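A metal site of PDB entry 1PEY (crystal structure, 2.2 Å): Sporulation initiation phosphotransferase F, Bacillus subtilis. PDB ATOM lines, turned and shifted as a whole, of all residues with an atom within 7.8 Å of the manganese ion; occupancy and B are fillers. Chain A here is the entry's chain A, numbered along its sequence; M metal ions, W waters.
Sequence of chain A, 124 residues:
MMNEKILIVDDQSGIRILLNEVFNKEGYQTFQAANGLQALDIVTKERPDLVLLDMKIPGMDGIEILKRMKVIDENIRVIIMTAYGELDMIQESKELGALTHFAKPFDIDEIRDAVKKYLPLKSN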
ATOM      1  N   VAL A   9       5.321  30.147  15.849  1.00  0.00           N
ATOM      2  CA  VAL A   9       5.920  31.194  16.678  1.00  0.00           C
ATOM      3  C   VAL A   9       6.591  30.589  17.911  1.00  0.00           C
ATOM      4  O   VAL A   9       5.918  30.045  18.786  1.00  0.00           O
ATOM      5  CB  VAL A   9       4.836  32.218  17.118  1.00  0.00           C
ATOM      6  CG1 VAL A   9       5.492  33.441  17.737  1.00  0.00           C
ATOM      7  CG2 VAL A   9       3.972  32.617  15.929  1.00  0.00           C
ATOM      8  N   ASP A  10       7.920  30.682  17.960  1.00  0.00           N
ATOM      9  CA  ASP A  10       8.712  30.145  19.073  1.00  0.00           C
ATOM     10  C   ASP A  10      10.097  30.819  19.066  1.00  0.00           C
ATOM     11  O   ASP A  10      10.754  30.893  18.025  1.00  0.00           O
ATOM     12  CB  ASP A  10       8.878  28.629  18.903  1.00  0.00           C
ATOM     13  CG  ASP A  10       9.282  27.944  20.192  1.00  0.00           C
ATOM     14  OD1 ASP A  10      10.425  28.128  20.664  1.00  0.00           O
ATOM     15  OD2 ASP A  10       8.439  27.194  20.734  1.00  0.00           O
ATOM     16  N   ASP A  11      10.525  31.289  20.235  1.00  0.00           N
ATOM     17  CA  ASP A  11      11.810  31.967  20.356  1.00  0.00           C
ATOM     18  C   ASP A  11      13.026  31.071  20.237  1.00  0.00           C
ATOM     19  O   ASP A  11      14.130  31.566  20.010  1.00  0.00           O
ATOM     20  CB  ASP A  11      11.872  32.752  21.672  1.00  0.00           C
ATOM     21  CG  ASP A  11      11.670  31.867  22.886  1.00  0.00           C
ATOM     22  OD1 ASP A  11      10.746  31.041  22.882  1.00  0.00           O
ATOM     23  OD2 ASP A  11      12.440  31.993  23.859  1.00  0.00           O
ATOM     24  N   GLN A  12      12.835  29.757  20.373  1.00  0.00           N
ATOM     25  CA  GLN A  12      13.950  28.828  20.261  1.00  0.00           C
ATOM     26  C   GLN A  12      14.043  28.172  18.889  1.00  0.00           C
ATOM     27  O   GLN A  12      13.241  27.313  18.520  1.00  0.00           O
ATOM     28  CB  GLN A  12      13.846  27.763  21.351  1.00  0.00           C
ATOM     29  CG  GLN A  12      14.058  28.358  22.723  1.00  0.00           C
ATOM     30  CD  GLN A  12      14.022  27.325  23.820  1.00  0.00           C
ATOM     31  OE1 GLN A  12      12.965  26.790  24.149  1.00  0.00           O
ATOM     32  NE2 GLN A  12      15.187  27.044  24.397  1.00  0.00           N
ATOM     33  N   ILE A  15      13.691  24.196  18.226  1.00  0.00           N
ATOM     34  CA  ILE A  15      12.317  23.747  18.251  1.00  0.00           C
ATOM     35  C   ILE A  15      11.476  24.344  17.109  1.00  0.00           C
ATOM     36  O   ILE A  15      10.708  23.635  16.469  1.00  0.00           O
ATOM     37  CB  ILE A  15      11.695  24.082  19.626  1.00  0.00           C
ATOM     38  CG1 ILE A  15      12.244  23.091  20.653  1.00  0.00           C
ATOM     39  CG2 ILE A  15      10.185  24.038  19.581  1.00  0.00           C
ATOM     40  CD1 ILE A  15      11.660  23.298  22.021  1.00  0.00           C
ATOM     41  N   ALA A  34      10.054  34.578  15.663  1.00  0.00           N
ATOM     42  CA  ALA A  34      10.776  34.358  16.913  1.00  0.00           C
ATOM     43  C   ALA A  34      10.217  35.143  18.088  1.00  0.00           C
ATOM     44  O   ALA A  34      10.618  34.941  19.236  1.00  0.00           O
ATOM     45  CB  ALA A  34      12.260  34.695  16.720  1.00  0.00           C
ATOM     46  N   ASP A  54       3.994  29.792  20.859  1.00  0.00           N
ATOM     47  CA  ASP A  54       4.742  29.507  22.069  1.00  0.00           C
ATOM     48  C   ASP A  54       4.374  30.627  23.032  1.00  0.00           C
ATOM     49  O   ASP A  54       4.629  31.806  22.755  1.00  0.00           O
ATOM     50  CB  ASP A  54       6.252  29.504  21.788  1.00  0.00           C
ATOM     51  CG  ASP A  54       7.083  29.533  23.054  1.00  0.00           C
ATOM     52  OD1 ASP A  54       6.602  29.069  24.120  1.00  0.00           O
ATOM     53  OD2 ASP A  54       8.233  30.012  22.988  1.00  0.00           O
ATOM     54  N   MET A  55       3.742  30.273  24.145  1.00  0.00           N
ATOM     55  CA  MET A  55       3.306  31.262  25.109  1.00  0.00           C
ATOM     56  C   MET A  55       4.388  31.787  26.037  1.00  0.00           C
ATOM     57  O   MET A  55       4.151  32.694  26.832  1.00  0.00           O
ATOM     58  CB  MET A  55       2.140  30.713  25.945  1.00  0.00           C
ATOM     59  CG  MET A  55       0.888  30.365  25.134  1.00  0.00           C
ATOM     60  SD  MET A  55       0.197  31.772  24.219  1.00  0.00           S
ATOM     61  CE  MET A  55      -0.858  32.540  25.477  1.00  0.00           C
ATOM     62  N   LYS A  56       5.591  31.230  25.933  1.00  0.00           N
ATOM     63  CA  LYS A  56       6.711  31.665  26.769  1.00  0.00           C
ATOM     64  C   LYS A  56       7.902  32.174  25.952  1.00  0.00           C
ATOM     65  O   LYS A  56       8.869  31.439  25.690  1.00  0.00           O
ATOM     66  CB  LYS A  56       7.166  30.523  27.700  1.00  0.00           C
ATOM     67  CG  LYS A  56       6.803  30.720  29.182  1.00  0.00           C
ATOM     68  CD  LYS A  56       5.306  30.573  29.462  1.00  0.00           C
ATOM     69  CE  LYS A  56       4.822  29.135  29.291  1.00  0.00           C
ATOM     70  NZ  LYS A  56       3.389  28.959  29.661  1.00  0.00           N
ATOM     71  N   ILE A  57       7.815  33.436  25.554  1.00  0.00           N
ATOM     72  CA  ILE A  57       8.836  34.123  24.773  1.00  0.00           C
ATOM     73  C   ILE A  57       9.158  35.372  25.603  1.00  0.00           C
ATOM     74  O   ILE A  57       8.259  36.150  25.912  1.00  0.00           O
ATOM     75  CB  ILE A  57       8.277  34.541  23.379  1.00  0.00           C
ATOM     76  CG1 ILE A  57       8.053  33.284  22.516  1.00  0.00           C
ATOM     77  CG2 ILE A  57       9.216  35.514  22.695  1.00  0.00           C
ATOM     78  CD1 ILE A  57       7.595  33.587  21.085  1.00  0.00           C
ATOM     79  N   PRO A  58      10.437  35.583  25.988  1.00  0.00           N
ATOM     80  CA  PRO A  58      10.754  36.770  26.799  1.00  0.00           C
ATOM     81  C   PRO A  58      10.253  38.105  26.242  1.00  0.00           C
ATOM     82  O   PRO A  58      10.500  38.440  25.078  1.00  0.00           O
ATOM     83  CB  PRO A  58      12.275  36.784  26.887  1.00  0.00           C
ATOM     84  CG  PRO A  58      12.714  35.440  26.459  1.00  0.00           C
ATOM     85  CD  PRO A  58      11.649  34.879  25.550  1.00  0.00           C
ATOM     86  N   MET A  81       1.115  26.819  22.956  1.00  0.00           N
ATOM     87  CA  MET A  81       2.124  25.924  23.514  1.00  0.00           C
ATOM     88  C   MET A  81       2.561  26.511  24.838  1.00  0.00           C
ATOM     89  O   MET A  81       3.013  27.670  24.907  1.00  0.00           O
ATOM     90  CB  MET A  81       3.318  25.795  22.569  1.00  0.00           C
ATOM     91  CG  MET A  81       2.931  25.284  21.184  1.00  0.00           C
ATOM     92  SD  MET A  81       4.370  24.910  20.097  1.00  0.00           S
ATOM     93  CE  MET A  81       4.990  26.537  19.586  1.00  0.00           C
ATOM     94  N   LYS A 104       5.140  21.739  26.722  1.00  0.00           N
ATOM     95  CA  LYS A 104       6.460  21.346  26.274  1.00  0.00           C
ATOM     96  C   LYS A 104       7.110  20.642  27.454  1.00  0.00           C
ATOM     97  O   LYS A 104       6.785  20.931  28.596  1.00  0.00           O
ATOM     98  CB  LYS A 104       7.307  22.575  25.945  1.00  0.00           C
ATOM     99  CG  LYS A 104       6.921  23.287  24.672  1.00  0.00           C
ATOM    100  CD  LYS A 104       7.868  24.461  24.465  1.00  0.00           C
ATOM    101  CE  LYS A 104       7.630  25.157  23.130  1.00  0.00           C
ATOM    102  NZ  LYS A 104       8.400  26.427  23.112  1.00  0.00           N
HETATM  103 MN    MN M   1       9.838  29.757  24.384  1.00  0.00          MN
HETATM  104  O   HOH W   1       9.117  27.794  25.911  1.00  0.00           O
HETATM  105  O   HOH W   2      11.727  29.840  25.715  1.00  0.00           O
HETATM  106  O   HOH W   3      10.729  27.997  23.301  1.00  0.00           O
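The manganese ion is bound by OD2 of Asp 54 (2.1 Å).
The manganese ion is bound by OD1 of Asp 11, 2.2 Å away.
Water W3 binds the manganese ion, at 2.3 Å.
Water W2 is bound to the manganese ion, 2.3 Å away.
O of Lys 56 binds the manganese ion, 2.3 Å away.
Water W1 is bound to the manganese ion, 2.6 Å away.
The manganese ion has six donor atoms within binding distance.
OD1 of Asp 54 lies within salt-bridge range of NZ of Lys 104 (3.4 Å).
The backbone NH of Asp 54 is in hydrogen-bond range of the backbone carbonyl oxygen of Val 9.
The side-chain amino group (NZ) of Lys 104 lies within salt-bridge range of the side-chain carboxylate (OD2) of Asp 10 (2.5 Å).
Lys 104 touches the manganese ion (NZ to MN, 3.8 Å).
Within 4 Å of the manganese ion: Asp 11, Asp 54, Lys 56 and Lys 104.
Along chain A the residues within 4 Å of the manganese ion span positions 11 to 104.
Water W1 bridges NZ of Lys 104 (3.2 Å) and OD1 of Asp 54 (3.3 Å).
Water W3 lies within hydrogen-bond range of OD1 of Asp 10 (2.7 Å), OE1 of Gln 12 (2.7 Å) and NZ of Lys 104 (2.8 Å).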
